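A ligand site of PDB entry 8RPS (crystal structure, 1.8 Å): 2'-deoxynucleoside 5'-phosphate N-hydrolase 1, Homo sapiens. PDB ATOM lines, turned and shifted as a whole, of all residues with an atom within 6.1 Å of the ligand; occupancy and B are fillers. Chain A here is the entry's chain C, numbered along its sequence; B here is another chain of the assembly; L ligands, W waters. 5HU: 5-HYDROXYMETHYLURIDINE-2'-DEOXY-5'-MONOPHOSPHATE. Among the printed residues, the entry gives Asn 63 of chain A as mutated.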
ATOM      1  N   TYR A   7      -1.986 -18.377 -13.075  1.00  0.00           N
ATOM      2  CA  TYR A   7      -2.165 -19.664 -12.427  1.00  0.00           C
ATOM      3  C   TYR A   7      -1.390 -19.682 -11.115  1.00  0.00           C
ATOM      4  O   TYR A   7      -0.198 -19.370 -11.085  1.00  0.00           O
ATOM      5  CB  TYR A   7      -1.678 -20.790 -13.341  1.00  0.00           C
ATOM      6  CG  TYR A   7      -1.754 -22.136 -12.710  1.00  0.00           C
ATOM      7  CD1 TYR A   7      -2.975 -22.711 -12.402  1.00  0.00           C
ATOM      8  CD2 TYR A   7      -0.593 -22.831 -12.400  1.00  0.00           C
ATOM      9  CE1 TYR A   7      -3.037 -23.970 -11.793  1.00  0.00           C
ATOM     10  CE2 TYR A   7      -0.648 -24.078 -11.800  1.00  0.00           C
ATOM     11  CZ  TYR A   7      -1.871 -24.641 -11.511  1.00  0.00           C
ATOM     12  OH  TYR A   7      -1.908 -25.874 -10.910  1.00  0.00           O
ATOM     13  N   PHE A   8      -2.066 -20.037 -10.012  1.00  0.00           N
ATOM     14  CA  PHE A   8      -1.384 -20.152  -8.737  1.00  0.00           C
ATOM     15  C   PHE A   8      -1.357 -21.596  -8.257  1.00  0.00           C
ATOM     16  O   PHE A   8      -2.379 -22.292  -8.295  1.00  0.00           O
ATOM     17  CB  PHE A   8      -2.015 -19.319  -7.637  1.00  0.00           C
ATOM     18  CG  PHE A   8      -1.345 -19.524  -6.300  1.00  0.00           C
ATOM     19  CD1 PHE A   8      -0.074 -19.002  -6.051  1.00  0.00           C
ATOM     20  CD2 PHE A   8      -1.931 -20.320  -5.320  1.00  0.00           C
ATOM     21  CE1 PHE A   8       0.559 -19.222  -4.856  1.00  0.00           C
ATOM     22  CE2 PHE A   8      -1.296 -20.550  -4.125  1.00  0.00           C
ATOM     23  CZ  PHE A   8      -0.043 -19.990  -3.883  1.00  0.00           C
ATOM     24  N   CYS A   9      -0.193 -22.058  -7.806  1.00  0.00           N
ATOM     25  CA  CYS A   9      -0.120 -23.429  -7.239  1.00  0.00           C
ATOM     26  C   CYS A   9       0.628 -23.464  -5.908  1.00  0.00           C
ATOM     27  O   CYS A   9       1.667 -22.804  -5.774  1.00  0.00           O
ATOM     28  CB  CYS A   9       0.541 -24.460  -8.137  1.00  0.00           C
ATOM     29  SG  CYS A   9       1.988 -23.884  -9.051  1.00  0.00           S
ATOM     30  N   GLY A  10       0.088 -24.235  -4.986  1.00  0.00           N
ATOM     31  CA  GLY A  10       0.724 -24.424  -3.688  1.00  0.00           C
ATOM     32  C   GLY A  10       0.468 -25.832  -3.220  1.00  0.00           C
ATOM     33  O   GLY A  10      -0.374 -26.501  -3.811  1.00  0.00           O
ATOM     34  N   SER A  11       1.185 -26.264  -2.196  1.00  0.00           N
ATOM     35  CA  SER A  11       1.057 -27.649  -1.708  1.00  0.00           C
ATOM     36  C   SER A  11      -0.358 -27.923  -1.199  1.00  0.00           C
ATOM     37  O   SER A  11      -0.976 -26.998  -0.723  1.00  0.00           O
ATOM     38  CB  SER A  11       2.022 -27.896  -0.591  1.00  0.00           C
ATOM     39  OG  SER A  11       1.852 -29.175  -0.013  1.00  0.00           O
ATOM     40  N   ILE A  12      -0.798 -29.174  -1.277  1.00  0.00           N
ATOM     41  CA  ILE A  12      -2.089 -29.606  -0.674  1.00  0.00           C
ATOM     42  C   ILE A  12      -1.785 -30.916   0.065  1.00  0.00           C
ATOM     43  O   ILE A  12      -1.635 -30.868   1.283  1.00  0.00           O
ATOM     44  CB  ILE A  12      -3.211 -29.746  -1.714  1.00  0.00           C
ATOM     45  CG1 ILE A  12      -3.489 -28.415  -2.411  1.00  0.00           C
ATOM     46  CG2 ILE A  12      -4.454 -30.318  -1.054  1.00  0.00           C
ATOM     47  CD1 ILE A  12      -4.620 -28.459  -3.402  1.00  0.00           C
ATOM     48  N   ARG A  13      -1.621 -32.011  -0.680  1.00  0.00           N
ATOM     49  CA  ARG A  13      -1.280 -33.349  -0.105  1.00  0.00           C
ATOM     50  C   ARG A  13       0.153 -33.374   0.423  1.00  0.00           C
ATOM     51  O   ARG A  13       0.453 -34.214   1.275  1.00  0.00           O
ATOM     52  CB  ARG A  13      -1.668 -34.487  -1.047  1.00  0.00           C
ATOM     53  CG  ARG A  13      -3.181 -34.675  -1.121  1.00  0.00           C
ATOM     54  CD  ARG A  13      -3.619 -35.818  -2.002  1.00  0.00           C
ATOM     55  NE  ARG A  13      -5.064 -35.836  -2.102  1.00  0.00           N
ATOM     56  CZ  ARG A  13      -5.726 -36.378  -3.105  1.00  0.00           C
ATOM     57  NH1 ARG A  13      -5.076 -36.952  -4.092  1.00  0.00           N
ATOM     58  NH2 ARG A  13      -7.051 -36.339  -3.121  1.00  0.00           N
ATOM     59  N   GLY A  14       1.026 -32.492  -0.093  1.00  0.00           N
ATOM     60  CA  GLY A  14       2.394 -32.302   0.406  1.00  0.00           C
ATOM     61  C   GLY A  14       2.370 -31.755   1.832  1.00  0.00           C
ATOM     62  O   GLY A  14       3.318 -32.012   2.577  1.00  0.00           O
ATOM     63  N   GLY A  15       1.360 -30.955   2.142  1.00  0.00           N
ATOM     64  CA  GLY A  15       1.089 -30.345   3.457  1.00  0.00           C
ATOM     65  C   GLY A  15       0.371 -29.020   3.289  1.00  0.00           C
ATOM     66  O   GLY A  15       0.695 -28.291   2.346  1.00  0.00           O
ATOM     67  N   GLU A  38      -6.716 -23.856  -7.598  1.00  0.00           N
ATOM     68  CA  GLU A  38      -7.569 -24.792  -6.907  1.00  0.00           C
ATOM     69  C   GLU A  38      -8.270 -24.123  -5.730  1.00  0.00           C
ATOM     70  O   GLU A  38      -7.627 -23.433  -4.924  1.00  0.00           O
ATOM     71  CB  GLU A  38      -6.756 -25.986  -6.396  1.00  0.00           C
ATOM     72  CG  GLU A  38      -7.603 -26.955  -5.558  1.00  0.00           C
ATOM     73  CD  GLU A  38      -8.529 -27.810  -6.425  1.00  0.00           C
ATOM     74  OE1 GLU A  38      -8.926 -27.347  -7.511  1.00  0.00           O
ATOM     75  OE2 GLU A  38      -8.838 -28.956  -6.023  1.00  0.00           O
ATOM     76  N   HIS A  39      -9.557 -24.419  -5.586  1.00  0.00           N
ATOM     77  CA  HIS A  39     -10.271 -24.036  -4.345  1.00  0.00           C
ATOM     78  C   HIS A  39     -10.145 -25.273  -3.466  1.00  0.00           C
ATOM     79  O   HIS A  39     -10.653 -26.331  -3.877  1.00  0.00           O
ATOM     80  CB  HIS A  39     -11.740 -23.685  -4.612  1.00  0.00           C
ATOM     81  CG  HIS A  39     -12.556 -23.703  -3.365  1.00  0.00           C
ATOM     82  ND1 HIS A  39     -13.081 -24.845  -2.819  1.00  0.00           N
ATOM     83  CD2 HIS A  39     -12.915 -22.704  -2.555  1.00  0.00           C
ATOM     84  CE1 HIS A  39     -13.748 -24.542  -1.716  1.00  0.00           C
ATOM     85  NE2 HIS A  39     -13.666 -23.241  -1.538  1.00  0.00           N
ATOM     86  N   ASP A  56      -9.019 -37.766  -8.835  1.00  0.00           N
ATOM     87  CA  ASP A  56      -7.716 -37.195  -9.145  1.00  0.00           C
ATOM     88  C   ASP A  56      -7.565 -36.860 -10.623  1.00  0.00           C
ATOM     89  O   ASP A  56      -6.887 -35.869 -10.975  1.00  0.00           O
ATOM     90  CB  ASP A  56      -6.587 -38.135  -8.696  1.00  0.00           C
ATOM     91  CG  ASP A  56      -6.485 -38.259  -7.172  1.00  0.00           C
ATOM     92  OD1 ASP A  56      -7.093 -37.438  -6.435  1.00  0.00           O
ATOM     93  OD2 ASP A  56      -5.762 -39.160  -6.704  1.00  0.00           O
ATOM     94  N   ILE A  59      -8.933 -33.479 -11.276  1.00  0.00           N
ATOM     95  CA  ILE A  59      -8.058 -32.475 -10.696  1.00  0.00           C
ATOM     96  C   ILE A  59      -6.836 -32.244 -11.588  1.00  0.00           C
ATOM     97  O   ILE A  59      -6.445 -31.105 -11.851  1.00  0.00           O
ATOM     98  CB  ILE A  59      -7.654 -32.876  -9.273  1.00  0.00           C
ATOM     99  CG1 ILE A  59      -8.898 -32.795  -8.362  1.00  0.00           C
ATOM    100  CG2 ILE A  59      -6.524 -31.966  -8.775  1.00  0.00           C
ATOM    101  CD1 ILE A  59      -8.747 -33.506  -7.024  1.00  0.00           C
ATOM    102  N   ASN A  63      -6.123 -28.543 -13.530  1.00  0.00           N
ATOM    103  CA  ASN A  63      -4.901 -27.783 -13.308  1.00  0.00           C
ATOM    104  C   ASN A  63      -4.043 -27.715 -14.561  1.00  0.00           C
ATOM    105  O   ASN A  63      -3.392 -26.696 -14.829  1.00  0.00           O
ATOM    106  CB  ASN A  63      -4.100 -28.374 -12.160  1.00  0.00           C
ATOM    107  CG  ASN A  63      -4.621 -27.941 -10.816  1.00  0.00           C
ATOM    108  OD1 ASN A  63      -4.213 -26.893 -10.295  1.00  0.00           O
ATOM    109  ND2 ASN A  63      -5.487 -28.759 -10.215  1.00  0.00           N
ATOM    110  N   TRP A  66      -5.643 -25.034 -16.761  1.00  0.00           N
ATOM    111  CA  TRP A  66      -5.386 -23.694 -16.190  1.00  0.00           C
ATOM    112  C   TRP A  66      -3.942 -23.262 -16.454  1.00  0.00           C
ATOM    113  O   TRP A  66      -3.723 -22.123 -16.866  1.00  0.00           O
ATOM    114  CB  TRP A  66      -5.659 -23.727 -14.693  1.00  0.00           C
ATOM    115  CG  TRP A  66      -7.115 -23.800 -14.345  1.00  0.00           C
ATOM    116  CD1 TRP A  66      -8.170 -23.370 -15.093  1.00  0.00           C
ATOM    117  CD2 TRP A  66      -7.671 -24.346 -13.131  1.00  0.00           C
ATOM    118  NE1 TRP A  66      -9.345 -23.620 -14.435  1.00  0.00           N
ATOM    119  CE2 TRP A  66      -9.076 -24.211 -13.238  1.00  0.00           C
ATOM    120  CE3 TRP A  66      -7.128 -24.928 -11.988  1.00  0.00           C
ATOM    121  CZ2 TRP A  66      -9.922 -24.634 -12.219  1.00  0.00           C
ATOM    122  CZ3 TRP A  66      -7.974 -25.348 -10.989  1.00  0.00           C
ATOM    123  CH2 TRP A  66      -9.349 -25.207 -11.105  1.00  0.00           C
ATOM    124  N   PRO A  80       7.540 -28.850   0.341  1.00  0.00           N
ATOM    125  CA  PRO A  80       7.751 -29.820  -0.756  1.00  0.00           C
ATOM    126  C   PRO A  80       6.453 -30.509  -1.140  1.00  0.00           C
ATOM    127  O   PRO A  80       5.653 -30.905  -0.300  1.00  0.00           O
ATOM    128  CB  PRO A  80       8.766 -30.809  -0.149  1.00  0.00           C
ATOM    129  CG  PRO A  80       9.481 -29.977   0.940  1.00  0.00           C
ATOM    130  CD  PRO A  80       8.328 -29.181   1.523  1.00  0.00           C
ATOM    131  N   SER A  81       6.239 -30.643  -2.455  1.00  0.00           N
ATOM    132  CA  SER A  81       4.959 -31.112  -2.960  1.00  0.00           C
ATOM    133  C   SER A  81       5.172 -31.739  -4.326  1.00  0.00           C
ATOM    134  O   SER A  81       5.758 -31.096  -5.200  1.00  0.00           O
ATOM    135  CB  SER A  81       3.956 -29.946  -3.038  1.00  0.00           C
ATOM    136  OG  SER A  81       2.935 -30.175  -4.008  1.00  0.00           O
ATOM    137  N   LEU A  82       4.711 -32.984  -4.503  1.00  0.00           N
ATOM    138  CA  LEU A  82       4.795 -33.579  -5.835  1.00  0.00           C
ATOM    139  C   LEU A  82       3.984 -32.789  -6.834  1.00  0.00           C
ATOM    140  O   LEU A  82       4.412 -32.564  -7.965  1.00  0.00           O
ATOM    141  CB  LEU A  82       4.295 -35.034  -5.829  1.00  0.00           C
ATOM    142  CG  LEU A  82       5.141 -35.997  -4.997  1.00  0.00           C
ATOM    143  CD1 LEU A  82       4.318 -37.225  -4.614  1.00  0.00           C
ATOM    144  CD2 LEU A  82       6.429 -36.348  -5.772  1.00  0.00           C
ATOM    145  N   GLY A  83       2.763 -32.408  -6.439  1.00  0.00           N
ATOM    146  CA  GLY A  83       1.877 -31.751  -7.379  1.00  0.00           C
ATOM    147  C   GLY A  83       2.413 -30.411  -7.827  1.00  0.00           C
ATOM    148  O   GLY A  83       2.313 -30.054  -8.998  1.00  0.00           O
ATOM    149  N   VAL A  84       2.998 -29.642  -6.902  1.00  0.00           N
ATOM    150  CA  VAL A  84       3.524 -28.358  -7.315  1.00  0.00           C
ATOM    151  C   VAL A  84       4.712 -28.561  -8.246  1.00  0.00           C
ATOM    152  O   VAL A  84       4.850 -27.873  -9.260  1.00  0.00           O
ATOM    153  CB  VAL A  84       3.909 -27.504  -6.088  1.00  0.00           C
ATOM    154  CG1 VAL A  84       4.663 -26.240  -6.557  1.00  0.00           C
ATOM    155  CG2 VAL A  84       2.666 -27.125  -5.291  1.00  0.00           C
ATOM    156  N   GLU A  87       3.393 -29.601 -11.675  1.00  0.00           N
ATOM    157  CA  GLU A  87       2.871 -28.430 -12.394  1.00  0.00           C
ATOM    158  C   GLU A  87       4.003 -27.565 -12.924  1.00  0.00           C
ATOM    159  O   GLU A  87       3.931 -27.092 -14.075  1.00  0.00           O
ATOM    160  CB  GLU A  87       1.939 -27.672 -11.466  1.00  0.00           C
ATOM    161  CG  GLU A  87       0.729 -28.553 -11.156  1.00  0.00           C
ATOM    162  CD  GLU A  87      -0.152 -28.050 -10.022  1.00  0.00           C
ATOM    163  OE1 GLU A  87       0.347 -27.305  -9.138  1.00  0.00           O
ATOM    164  OE2 GLU A  87      -1.323 -28.468  -9.962  1.00  0.00           O
ATOM    165  N   LEU B 110      -1.324 -39.884  -1.868  1.00  0.00           N
ATOM    166  CA  LEU B 110      -0.543 -39.492  -3.029  1.00  0.00           C
ATOM    167  C   LEU B 110      -1.207 -38.320  -3.735  1.00  0.00           C
ATOM    168  O   LEU B 110      -2.429 -38.331  -3.968  1.00  0.00           O
ATOM    169  CB  LEU B 110      -0.394 -40.661  -4.002  1.00  0.00           C
ATOM    170  CG  LEU B 110       0.378 -40.372  -5.283  1.00  0.00           C
ATOM    171  CD1 LEU B 110       1.791 -39.903  -4.931  1.00  0.00           C
ATOM    172  CD2 LEU B 110       0.420 -41.622  -6.172  1.00  0.00           C
ATOM    173  N   SER B 111      -0.400 -37.315  -4.067  1.00  0.00           N
ATOM    174  CA  SER B 111      -0.805 -36.163  -4.869  1.00  0.00           C
ATOM    175  C   SER B 111      -1.788 -36.535  -5.973  1.00  0.00           C
ATOM    176  O   SER B 111      -1.545 -37.468  -6.745  1.00  0.00           O
ATOM    177  CB  SER B 111       0.448 -35.542  -5.485  1.00  0.00           C
ATOM    178  OG  SER B 111       0.114 -34.490  -6.378  1.00  0.00           O
ATOM    179  N   ALA B 112      -2.865 -35.750  -6.085  1.00  0.00           N
ATOM    180  CA  ALA B 112      -3.811 -35.952  -7.173  1.00  0.00           C
ATOM    181  C   ALA B 112      -3.170 -35.672  -8.534  1.00  0.00           C
ATOM    182  O   ALA B 112      -3.616 -36.221  -9.541  1.00  0.00           O
ATOM    183  CB  ALA B 112      -5.025 -35.050  -6.962  1.00  0.00           C
ATOM    184  N   MET B 113      -2.095 -34.885  -8.579  1.00  0.00           N
ATOM    185  CA  MET B 113      -1.458 -34.583  -9.857  1.00  0.00           C
ATOM    186  C   MET B 113      -0.692 -35.782 -10.380  1.00  0.00           C
ATOM    187  O   MET B 113      -0.545 -35.935 -11.591  1.00  0.00           O
ATOM    188  CB  MET B 113      -0.515 -33.403  -9.683  1.00  0.00           C
ATOM    189  CG  MET B 113      -1.191 -32.034  -9.577  1.00  0.00           C
ATOM    190  SD  MET B 113      -2.618 -31.773 -10.636  1.00  0.00           S
ATOM    191  CE  MET B 113      -1.813 -31.193 -12.112  1.00  0.00           C
HETATM  192  P   5HU L   1       0.052 -31.762  -3.827  1.00  0.00           P
HETATM  193  OP1 5HU L   1       0.708 -31.038  -2.706  1.00  0.00           O
HETATM  194  OP2 5HU L   1       0.880 -32.915  -4.267  1.00  0.00           O
HETATM  195  OP3 5HU L   1      -1.301 -32.239  -3.428  1.00  0.00           O
HETATM  196  O5' 5HU L   1      -0.128 -30.756  -5.098  1.00  0.00           O
HETATM  197  C5' 5HU L   1      -0.746 -29.526  -4.915  1.00  0.00           C
HETATM  198  C4' 5HU L   1      -1.028 -28.919  -6.302  1.00  0.00           C
HETATM  199  O4' 5HU L   1      -1.743 -30.006  -7.183  1.00  0.00           O
HETATM  200  C3' 5HU L   1      -1.842 -27.926  -6.198  1.00  0.00           C
HETATM  201  O3' 5HU L   1      -1.162 -26.700  -6.538  1.00  0.00           O
HETATM  202  C2' 5HU L   1      -3.019 -28.144  -7.294  1.00  0.00           C
HETATM  203  C1' 5HU L   1      -3.124 -29.434  -7.531  1.00  0.00           C
HETATM  204  N1  5HU L   1      -4.136 -30.039  -6.667  1.00  0.00           N
HETATM  205  C2  5HU L   1      -5.535 -29.581  -6.724  1.00  0.00           C
HETATM  206  O2  5HU L   1      -5.866 -28.747  -7.476  1.00  0.00           O
HETATM  207  N3  5HU L   1      -6.545 -30.197  -5.851  1.00  0.00           N
HETATM  208  C4  5HU L   1      -6.192 -31.248  -4.928  1.00  0.00           C
HETATM  209  O4  5HU L   1      -6.993 -31.732  -4.237  1.00  0.00           O
HETATM  210  C5  5HU L   1      -4.781 -31.713  -4.882  1.00  0.00           C
HETATM  211  C5A 5HU L   1      -4.395 -32.822  -3.925  1.00  0.00           C
HETATM  212  C6  5HU L   1      -3.769 -31.107  -5.756  1.00  0.00           C
HETATM  213  O5B 5HU L   1      -3.375 -33.564  -4.501  1.00  0.00           O
HETATM  214  O   HOH W   1       2.751 -34.063  -2.734  1.00  0.00           O
HETATM  215  O   HOH W   2      -9.528 -31.717  -4.106  1.00  0.00           O
HETATM  216  O   HOH W   3      -2.940 -24.803  -5.062  1.00  0.00           O
HETATM  217  O   HOH W   4      -7.175 -33.290  -1.705  1.00  0.00           O
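Water W2 lies within hydrogen-bond range of an oxygen (O4) of the ligand (2.5 Å) and the side-chain carboxylate of Glu 38 (3.4 Å). Water W1 bridges OP2 of the ligand (2.7 Å) and N of Leu 82 (2.9 Å). Water W4 lies within hydrogen-bond range of O4 of the ligand (3.0 Å) and NE of Arg 13 (3.3 Å). Water W3 lies within hydrogen-bond range of an oxygen (O3') of the ligand (3.0 Å) and the backbone NH (N) of Gly 10 (3.1 Å).
The guanidinium group (NH1) of Arg 13 lies within hydrogen-bond range of the backbone carbonyl oxygen (O) of Leu 110 of chain B (3.0 Å). NH1 of Arg 13 is in salt-bridge range of OD1 of Asp 56, 3.1 Å away. The side-chain hydroxyl of Ser 111 of chain B lies close to the backbone NH of Met 113 of chain B. The side-chain amide oxygen of Asn 63 is in hydrogen-bond range of the side-chain hydroxyl of Tyr 7. The side-chain hydroxyl of Ser 81 is in hydrogen-bond range of the backbone NH of Val 84 (2.9 Å). OE1 of Glu 87 sits close to SG of Cys 9 (3.8 Å). OH of Tyr 7 sits at hydrogen-bond distance from OE2 of Glu 87. The side-chain hydroxyl (OG) of Ser 11 lies within hydrogen-bond range of the backbone carbonyl oxygen (O) of Gly 15 (2.8 Å).
Merely in contact with the ligand: Cys 9 (3.2 Å), Ile 59 (3.3 Å), Leu 82 (3.8 Å), Val 84 (3.8 Å) and Met 113 of chain B (3.2 Å). 17 residues have an atom within 4 Å of the ligand: Cys 9, Gly 10, Ser 11, Ile 12, Arg 13, Gly 14, Glu 38, Ile 59, Asn 63, Ser 81, Leu 82, Gly 83, Val 84, Glu 87, Ser 111 of chain B, Ala 112 of chain B and Met 113 of chain B.
The side-chain carboxylate (OE2) of Glu 38 sits at hydrogen-bond distance from a nitrogen (N3) of the ligand. The backbone NH of Ile 12 lies within hydrogen-bond range of an oxygen (OP1) of the ligand (2.8 Å). N of Gly 14 lies within hydrogen-bond range of OP1 of the ligand (3.0 Å). The side-chain carboxylate (OE1) of Glu 87 is in hydrogen-bond range of an oxygen (O3') of the ligand, at 3.1 Å. O3' of the ligand sits at hydrogen-bond distance from N of Gly 10. The side-chain hydroxyl (OG) of Ser 81 is in hydrogen-bond range of an oxygen (OP1) of the ligand (2.7 Å). O2 of the ligand lies within hydrogen-bond range of ND2 of Asn 63, 2.8 Å away. The backbone NH of Arg 13 is in hydrogen-bond range of an oxygen (OP3) of the ligand. The side-chain hydroxyl of Ser 111 of chain B lies within hydrogen-bond range of an oxygen (OP2) of the ligand (2.7 Å). The backbone NH of Ala 112 of chain B is in hydrogen-bond range of an oxygen (O5B) of the ligand (2.7 Å). The side-chain hydroxyl (OG) of Ser 11 lies within hydrogen-bond range of an oxygen (OP1) of the ligand (3.5 Å). N of Gly 83 is in hydrogen-bond range of OP2 of the ligand. The backbone carbonyl oxygen of Gly 10 sits at hydrogen-bond distance from an oxygen (O3') of the ligand (2.8 Å).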
